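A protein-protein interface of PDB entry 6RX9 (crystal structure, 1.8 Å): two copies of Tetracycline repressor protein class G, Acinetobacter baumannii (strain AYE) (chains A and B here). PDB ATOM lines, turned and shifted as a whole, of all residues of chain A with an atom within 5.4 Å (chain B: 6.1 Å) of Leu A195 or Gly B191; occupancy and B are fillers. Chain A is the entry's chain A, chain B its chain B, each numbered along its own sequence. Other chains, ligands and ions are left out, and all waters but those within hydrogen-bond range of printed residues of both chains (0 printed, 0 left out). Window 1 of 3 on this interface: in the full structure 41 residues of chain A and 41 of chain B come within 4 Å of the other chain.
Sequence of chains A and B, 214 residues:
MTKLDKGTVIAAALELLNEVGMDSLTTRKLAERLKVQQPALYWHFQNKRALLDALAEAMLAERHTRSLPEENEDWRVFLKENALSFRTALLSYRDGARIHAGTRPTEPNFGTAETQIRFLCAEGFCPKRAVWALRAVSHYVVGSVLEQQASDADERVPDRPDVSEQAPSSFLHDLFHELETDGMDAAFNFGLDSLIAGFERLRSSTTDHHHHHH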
ATOM      1  N   ALA A 136      26.328   0.691 -28.808  1.00  0.00           N
ATOM      2  CA  ALA A 136      24.894   0.632 -28.435  1.00  0.00           C
ATOM      3  C   ALA A 136      24.413   2.011 -27.963  1.00  0.00           C
ATOM      4  O   ALA A 136      23.316   2.428 -28.382  1.00  0.00           O
ATOM      5  CB  ALA A 136      24.666  -0.420 -27.382  1.00  0.00           C
ATOM      6  N   VAL A 137      25.202   2.693 -27.128  1.00  0.00           N
ATOM      7  CA  VAL A 137      24.891   4.066 -26.630  1.00  0.00           C
ATOM      8  C   VAL A 137      24.750   5.007 -27.838  1.00  0.00           C
ATOM      9  O   VAL A 137      23.745   5.743 -27.910  1.00  0.00           O
ATOM     10  CB  VAL A 137      25.943   4.562 -25.617  1.00  0.00           C
ATOM     11  CG1 VAL A 137      25.794   6.047 -25.319  1.00  0.00           C
ATOM     12  CG2 VAL A 137      25.893   3.756 -24.327  1.00  0.00           C
ATOM     13  N   TYR A 140      21.515   4.378 -29.895  1.00  0.00           N
ATOM     14  CA  TYR A 140      20.343   4.916 -29.157  1.00  0.00           C
ATOM     15  C   TYR A 140      20.244   6.434 -29.373  1.00  0.00           C
ATOM     16  O   TYR A 140      19.147   6.921 -29.701  1.00  0.00           O
ATOM     17  CB  TYR A 140      20.408   4.563 -27.668  1.00  0.00           C
ATOM     18  CG  TYR A 140      19.359   5.269 -26.851  1.00  0.00           C
ATOM     19  CD1 TYR A 140      18.023   4.914 -26.951  1.00  0.00           C
ATOM     20  CD2 TYR A 140      19.688   6.326 -26.019  1.00  0.00           C
ATOM     21  CE1 TYR A 140      17.044   5.576 -26.228  1.00  0.00           C
ATOM     22  CE2 TYR A 140      18.721   6.997 -25.288  1.00  0.00           C
ATOM     23  CZ  TYR A 140      17.393   6.624 -25.397  1.00  0.00           C
ATOM     24  OH  TYR A 140      16.432   7.276 -24.680  1.00  0.00           O
ATOM     25  N   PHE A 190      15.330   8.351 -19.741  1.00  0.00           N
ATOM     26  CA  PHE A 190      14.773   7.032 -19.336  1.00  0.00           C
ATOM     27  C   PHE A 190      15.440   5.913 -20.147  1.00  0.00           C
ATOM     28  O   PHE A 190      15.878   4.926 -19.535  1.00  0.00           O
ATOM     29  CB  PHE A 190      13.251   6.971 -19.465  1.00  0.00           C
ATOM     30  CG  PHE A 190      12.710   5.594 -19.187  1.00  0.00           C
ATOM     31  CD1 PHE A 190      12.585   5.134 -17.885  1.00  0.00           C
ATOM     32  CD2 PHE A 190      12.385   4.736 -20.226  1.00  0.00           C
ATOM     33  CE1 PHE A 190      12.112   3.856 -17.631  1.00  0.00           C
ATOM     34  CE2 PHE A 190      11.912   3.458 -19.969  1.00  0.00           C
ATOM     35  CZ  PHE A 190      11.775   3.022 -18.671  1.00  0.00           C
ATOM     36  N   GLY A 191      15.516   6.053 -21.475  1.00  0.00           N
ATOM     37  CA  GLY A 191      16.184   5.072 -22.352  1.00  0.00           C
ATOM     38  C   GLY A 191      17.667   4.939 -22.030  1.00  0.00           C
ATOM     39  O   GLY A 191      18.176   3.797 -22.025  1.00  0.00           O
ATOM     40  N   LEU A 192      18.346   6.064 -21.789  1.00  0.00           N
ATOM     41  CA  LEU A 192      19.806   6.107 -21.497  1.00  0.00           C
ATOM     42  C   LEU A 192      20.083   5.387 -20.171  1.00  0.00           C
ATOM     43  O   LEU A 192      20.976   4.520 -20.148  1.00  0.00           O
ATOM     44  CB  LEU A 192      20.270   7.566 -21.445  1.00  0.00           C
ATOM     45  CG  LEU A 192      21.754   7.784 -21.146  1.00  0.00           C
ATOM     46  CD1 LEU A 192      22.632   6.936 -22.053  1.00  0.00           C
ATOM     47  CD2 LEU A 192      22.111   9.254 -21.280  1.00  0.00           C
ATOM     48  N   ASP A 193      19.331   5.728 -19.121  1.00  0.00           N
ATOM     49  CA  ASP A 193      19.460   5.139 -17.759  1.00  0.00           C
ATOM     50  C   ASP A 193      19.189   3.630 -17.825  1.00  0.00           C
ATOM     51  O   ASP A 193      19.903   2.874 -17.140  1.00  0.00           O
ATOM     52  CB  ASP A 193      18.535   5.844 -16.765  1.00  0.00           C
ATOM     53  CG  ASP A 193      18.951   7.266 -16.430  1.00  0.00           C
ATOM     54  OD1 ASP A 193      20.109   7.631 -16.727  1.00  0.00           O
ATOM     55  OD2 ASP A 193      18.114   8.001 -15.870  1.00  0.00           O
ATOM     56  N   SER A 194      18.202   3.206 -18.623  1.00  0.00           N
ATOM     57  CA  SER A 194      17.847   1.779 -18.837  1.00  0.00           C
ATOM     58  C   SER A 194      19.014   1.048 -19.510  1.00  0.00           C
ATOM     59  O   SER A 194      19.383  -0.042 -19.043  1.00  0.00           O
ATOM     60  CB  SER A 194      16.575   1.643 -19.633  1.00  0.00           C
ATOM     61  OG  SER A 194      15.483   2.208 -18.920  1.00  0.00           O
ATOM     62  N   LEU A 195      19.585   1.629 -20.566  1.00  0.00           N
ATOM     63  CA  LEU A 195      20.727   1.032 -21.305  1.00  0.00           C
ATOM     64  C   LEU A 195      21.899   0.812 -20.334  1.00  0.00           C
ATOM     65  O   LEU A 195      22.438  -0.312 -20.295  1.00  0.00           O
ATOM     66  CB  LEU A 195      21.107   1.968 -22.457  1.00  0.00           C
ATOM     67  CG  LEU A 195      21.980   1.367 -23.559  1.00  0.00           C
ATOM     68  CD1 LEU A 195      21.401   0.061 -24.084  1.00  0.00           C
ATOM     69  CD2 LEU A 195      22.159   2.364 -24.698  1.00  0.00           C
ATOM     70  N   ILE A 196      22.258   1.836 -19.556  1.00  0.00           N
ATOM     71  CA  ILE A 196      23.434   1.802 -18.632  1.00  0.00           C
ATOM     72  C   ILE A 196      23.158   0.809 -17.491  1.00  0.00           C
ATOM     73  O   ILE A 196      24.072   0.027 -17.168  1.00  0.00           O
ATOM     74  CB  ILE A 196      23.785   3.219 -18.133  1.00  0.00           C
ATOM     75  CG1 ILE A 196      24.293   4.094 -19.284  1.00  0.00           C
ATOM     76  CG2 ILE A 196      24.783   3.165 -16.985  1.00  0.00           C
ATOM     77  CD1 ILE A 196      24.316   5.571 -18.978  1.00  0.00           C
ATOM     78  N   ALA A 197      21.951   0.824 -16.912  1.00  0.00           N
ATOM     79  CA  ALA A 197      21.520  -0.119 -15.849  1.00  0.00           C
ATOM     80  C   ALA A 197      21.659  -1.562 -16.352  1.00  0.00           C
ATOM     81  O   ALA A 197      22.095  -2.425 -15.565  1.00  0.00           O
ATOM     82  CB  ALA A 197      20.104   0.179 -15.420  1.00  0.00           C
ATOM     83  N   GLY A 198      21.299  -1.811 -17.615  1.00  0.00           N
ATOM     84  CA  GLY A 198      21.401  -3.128 -18.274  1.00  0.00           C
ATOM     85  C   GLY A 198      22.838  -3.596 -18.431  1.00  0.00           C
ATOM     86  O   GLY A 198      23.075  -4.809 -18.284  1.00  0.00           O
ATOM     87  N   PHE A 199      23.767  -2.685 -18.739  1.00  0.00           N
ATOM     88  CA  PHE A 199      25.213  -2.994 -18.893  1.00  0.00           C
ATOM     89  C   PHE A 199      25.760  -3.591 -17.591  1.00  0.00           C
ATOM     90  O   PHE A 199      26.561  -4.539 -17.676  1.00  0.00           O
ATOM     91  CB  PHE A 199      26.020  -1.754 -19.288  1.00  0.00           C
ATOM     92  CG  PHE A 199      25.736  -1.200 -20.663  1.00  0.00           C
ATOM     93  CD1 PHE A 199      25.304  -2.018 -21.698  1.00  0.00           C
ATOM     94  CD2 PHE A 199      25.934   0.146 -20.927  1.00  0.00           C
ATOM     95  CE1 PHE A 199      25.059  -1.494 -22.958  1.00  0.00           C
ATOM     96  CE2 PHE A 199      25.691   0.666 -22.189  1.00  0.00           C
ATOM     97  CZ  PHE A 199      25.254  -0.155 -23.201  1.00  0.00           C
ATOM     98  N   TYR B 140      16.830   2.721 -30.609  1.00  0.00           N
ATOM     99  CA  TYR B 140      18.009   1.815 -30.625  1.00  0.00           C
ATOM    100  C   TYR B 140      18.043   1.031 -31.946  1.00  0.00           C
ATOM    101  O   TYR B 140      19.124   0.939 -32.552  1.00  0.00           O
ATOM    102  CB  TYR B 140      18.011   0.862 -29.427  1.00  0.00           C
ATOM    103  CG  TYR B 140      19.071  -0.205 -29.533  1.00  0.00           C
ATOM    104  CD1 TYR B 140      20.411   0.113 -29.387  1.00  0.00           C
ATOM    105  CD2 TYR B 140      18.745  -1.519 -29.826  1.00  0.00           C
ATOM    106  CE1 TYR B 140      21.399  -0.850 -29.506  1.00  0.00           C
ATOM    107  CE2 TYR B 140      19.721  -2.496 -29.947  1.00  0.00           C
ATOM    108  CZ  TYR B 140      21.055  -2.159 -29.791  1.00  0.00           C
ATOM    109  OH  TYR B 140      22.030  -3.107 -29.906  1.00  0.00           O
ATOM    110  N   ALA B 186      25.189 -10.506 -32.873  1.00  0.00           N
ATOM    111  CA  ALA B 186      25.751 -10.534 -31.502  1.00  0.00           C
ATOM    112  C   ALA B 186      25.763  -9.114 -30.922  1.00  0.00           C
ATOM    113  O   ALA B 186      25.251  -8.928 -29.800  1.00  0.00           O
ATOM    114  CB  ALA B 186      27.134 -11.141 -31.520  1.00  0.00           C
ATOM    115  N   ALA B 187      26.320  -8.154 -31.666  1.00  0.00           N
ATOM    116  CA  ALA B 187      26.414  -6.723 -31.286  1.00  0.00           C
ATOM    117  C   ALA B 187      25.011  -6.154 -31.032  1.00  0.00           C
ATOM    118  O   ALA B 187      24.813  -5.501 -29.985  1.00  0.00           O
ATOM    119  CB  ALA B 187      27.135  -5.950 -32.362  1.00  0.00           C
ATOM    120  N   PHE B 188      24.070  -6.394 -31.947  1.00  0.00           N
ATOM    121  CA  PHE B 188      22.680  -5.881 -31.846  1.00  0.00           C
ATOM    122  C   PHE B 188      22.014  -6.440 -30.582  1.00  0.00           C
ATOM    123  O   PHE B 188      21.443  -5.646 -29.814  1.00  0.00           O
ATOM    124  CB  PHE B 188      21.848  -6.217 -33.086  1.00  0.00           C
ATOM    125  CG  PHE B 188      20.394  -5.863 -32.908  1.00  0.00           C
ATOM    126  CD1 PHE B 188      19.976  -4.542 -32.974  1.00  0.00           C
ATOM    127  CD2 PHE B 188      19.458  -6.838 -32.595  1.00  0.00           C
ATOM    128  CE1 PHE B 188      18.645  -4.210 -32.776  1.00  0.00           C
ATOM    129  CE2 PHE B 188      18.128  -6.502 -32.396  1.00  0.00           C
ATOM    130  CZ  PHE B 188      17.725  -5.191 -32.484  1.00  0.00           C
ATOM    131  N   ASN B 189      22.096  -7.759 -30.376  1.00  0.00           N
ATOM    132  CA  ASN B 189      21.424  -8.481 -29.260  1.00  0.00           C
ATOM    133  C   ASN B 189      21.947  -7.965 -27.914  1.00  0.00           C
ATOM    134  O   ASN B 189      21.135  -7.834 -26.986  1.00  0.00           O
ATOM    135  CB  ASN B 189      21.585  -9.998 -29.381  1.00  0.00           C
ATOM    136  CG  ASN B 189      20.827 -10.586 -30.553  1.00  0.00           C
ATOM    137  OD1 ASN B 189      19.788 -10.069 -30.957  1.00  0.00           O
ATOM    138  ND2 ASN B 189      21.340 -11.671 -31.108  1.00  0.00           N
ATOM    139  N   PHE B 190      23.249  -7.682 -27.806  1.00  0.00           N
ATOM    140  CA  PHE B 190      23.875  -7.182 -26.554  1.00  0.00           C
ATOM    141  C   PHE B 190      23.201  -5.869 -26.135  1.00  0.00           C
ATOM    142  O   PHE B 190      22.836  -5.735 -24.952  1.00  0.00           O
ATOM    143  CB  PHE B 190      25.387  -6.991 -26.706  1.00  0.00           C
ATOM    144  CG  PHE B 190      26.030  -6.373 -25.491  1.00  0.00           C
ATOM    145  CD1 PHE B 190      26.406  -7.159 -24.413  1.00  0.00           C
ATOM    146  CD2 PHE B 190      26.211  -5.001 -25.402  1.00  0.00           C
ATOM    147  CE1 PHE B 190      26.976  -6.586 -23.287  1.00  0.00           C
ATOM    148  CE2 PHE B 190      26.785  -4.433 -24.276  1.00  0.00           C
ATOM    149  CZ  PHE B 190      27.165  -5.226 -23.221  1.00  0.00           C
ATOM    150  N   GLY B 191      23.048  -4.927 -27.073  1.00  0.00           N
ATOM    151  CA  GLY B 191      22.413  -3.621 -26.816  1.00  0.00           C
ATOM    152  C   GLY B 191      20.951  -3.778 -26.433  1.00  0.00           C
ATOM    153  O   GLY B 191      20.520  -3.129 -25.461  1.00  0.00           O
ATOM    154  N   LEU B 192      20.215  -4.625 -27.160  1.00  0.00           N
ATOM    155  CA  LEU B 192      18.773  -4.898 -26.919  1.00  0.00           C
ATOM    156  C   LEU B 192      18.604  -5.568 -25.547  1.00  0.00           C
ATOM    157  O   LEU B 192      17.745  -5.107 -24.769  1.00  0.00           O
ATOM    158  CB  LEU B 192      18.234  -5.777 -28.053  1.00  0.00           C
ATOM    159  CG  LEU B 192      16.749  -6.134 -27.975  1.00  0.00           C
ATOM    160  CD1 LEU B 192      15.888  -4.886 -27.880  1.00  0.00           C
ATOM    161  CD2 LEU B 192      16.336  -6.977 -29.171  1.00  0.00           C
ATOM    162  N   ASP B 193      19.404  -6.599 -25.253  1.00  0.00           N
ATOM    163  CA  ASP B 193      19.357  -7.348 -23.965  1.00  0.00           C
ATOM    164  C   ASP B 193      19.637  -6.382 -22.806  1.00  0.00           C
ATOM    165  O   ASP B 193      18.974  -6.511 -21.757  1.00  0.00           O
ATOM    166  CB  ASP B 193      20.317  -8.544 -23.975  1.00  0.00           C
ATOM    167  CG  ASP B 193      19.888  -9.686 -24.886  1.00  0.00           C
ATOM    168  OD1 ASP B 193      18.714  -9.696 -25.320  1.00  0.00           O
ATOM    169  OD2 ASP B 193      20.735 -10.560 -25.162  1.00  0.00           O
ATOM    170  N   SER B 194      20.568  -5.441 -22.984  1.00  0.00           N
ATOM    171  CA  SER B 194      20.939  -4.419 -21.967  1.00  0.00           C
ATOM    172  C   SER B 194      19.755  -3.471 -21.723  1.00  0.00           C
ATOM    173  O   SER B 194      19.441  -3.203 -20.553  1.00  0.00           O
ATOM    174  CB  SER B 194      22.185  -3.672 -22.378  1.00  0.00           C
ATOM    175  OG  SER B 194      23.292  -4.557 -22.475  1.00  0.00           O
ATOM    176  N   LEU B 195      19.097  -2.999 -22.784  1.00  0.00           N
ATOM    177  CA  LEU B 195      17.936  -2.074 -22.683  1.00  0.00           C
ATOM    178  C   LEU B 195      16.815  -2.763 -21.885  1.00  0.00           C
ATOM    179  O   LEU B 195      16.291  -2.147 -20.926  1.00  0.00           O
ATOM    180  CB  LEU B 195      17.489  -1.698 -24.102  1.00  0.00           C
ATOM    181  CG  LEU B 195      16.600  -0.463 -24.228  1.00  0.00           C
ATOM    182  CD1 LEU B 195      17.265   0.771 -23.638  1.00  0.00           C
ATOM    183  CD2 LEU B 195      16.231  -0.220 -25.684  1.00  0.00           C
ATOM    184  N   ILE B 196      16.492  -4.009 -22.241  1.00  0.00           N
ATOM    185  CA  ILE B 196      15.390  -4.802 -21.617  1.00  0.00           C
ATOM    186  C   ILE B 196      15.752  -5.115 -20.157  1.00  0.00           C
ATOM    187  O   ILE B 196      14.871  -4.952 -19.289  1.00  0.00           O
ATOM    188  CB  ILE B 196      15.084  -6.067 -22.451  1.00  0.00           C
ATOM    189  CG1 ILE B 196      14.489  -5.692 -23.813  1.00  0.00           C
ATOM    190  CG2 ILE B 196      14.182  -7.025 -21.683  1.00  0.00           C
ATOM    191  CD1 ILE B 196      14.403  -6.841 -24.795  1.00  0.00           C
ATOM    192  N   GLY B 198      17.656  -3.354 -18.262  1.00  0.00           N
ATOM    193  CA  GLY B 198      17.582  -2.049 -17.580  1.00  0.00           C
ATOM    194  C   GLY B 198      16.159  -1.655 -17.223  1.00  0.00           C
ATOM    195  O   GLY B 198      15.979  -1.004 -16.179  1.00  0.00           O
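The side-chain hydroxyl (OG) of Ser A194 sits at hydrogen-bond distance from the backbone carbonyl oxygen (O) of Phe A190, at 2.8 Å. The backbone carbonyl oxygen of Phe B188 is in hydrogen-bond range of the side-chain hydroxyl of Tyr B140 (2.6 Å). The side-chain hydroxyl (OG) of Ser B194 lies within hydrogen-bond range of the backbone carbonyl oxygen (O) of Phe B190 (2.8 Å).
Among the printed residues, pairs that only touch across the chains: Gly A198 with Ser B194, Ser A194 with Gly B198, Phe A199 with Ser B194, Ser A194 with Ser B194, Gly A191 with Leu B195, Leu A195 with Gly B191, Phe A199 with Phe B190, Gly A198 with Gly B198, Ala A136 with Tyr B140, Leu A195 with Leu B195, Ala A136 with Gly B191, Leu A195 with Ser B194 and Ala A197 with Gly B198.
Gly B191 touches just these residues of chain A: Ala A136 (3.96 Å) and Leu A195 (3.6 Å). Printed residues of chain B within 4 Å of Ser A194: Ser B194 and Gly B198. Printed residues of chain B within 4 Å of Ala A136: Tyr B140 and Gly B191. Ala B186 touches none of the printed residues of chain A. Ile A196 touches none of the printed residues of chain B. The nearest residue of chain B that does not touch Leu A195 is Gly B198 (5.1 Å). The nearest residue of chain A that does not touch Gly B191 is Phe A199 (5.1 Å).
Hydrophobic or aromatic side chains of chain A within 4 Å of the printed part of chain B: Ala A136, Leu A195, Ala A197 and Phe A199. Of the 13 printed residues of chain B, 6 touch a printed residue of chain A. Printed residues of chain B that touch a printed residue of chain A: Tyr B140, Phe B190, Gly B191, Ser B194, Leu B195 and Gly B198. Hydrophobic or aromatic side chains of chain B within 4 Å of the printed part of chain A: Tyr B140, Phe B190 and Leu B195. Among the printed residues, 13 pairs touch across the chains. Among the printed residues, no Asp or Glu carboxylate lies within 4 Å of a Lys or Arg side-chain nitrogen of the other chain.
Gly A191 touches Leu B195, and with the chains exchanged Leu A195 touches Gly B191. Ser A194 touches Gly B198, and with the chains exchanged Gly A198 touches Ser B194. Leu A195 touches Ser B194, but with the chains exchanged Ser A194 does not touch Leu B195 (4.01 Å). Leu A195 touches its own counterpart, Leu B195. Positions printed for both chains: 140, 190, 191, 192, 193, 194, 195, 196 and 198. Of the 13 pairs that touch across the chains among the printed residues, 7 have their exchanged pair printed and touching as well.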
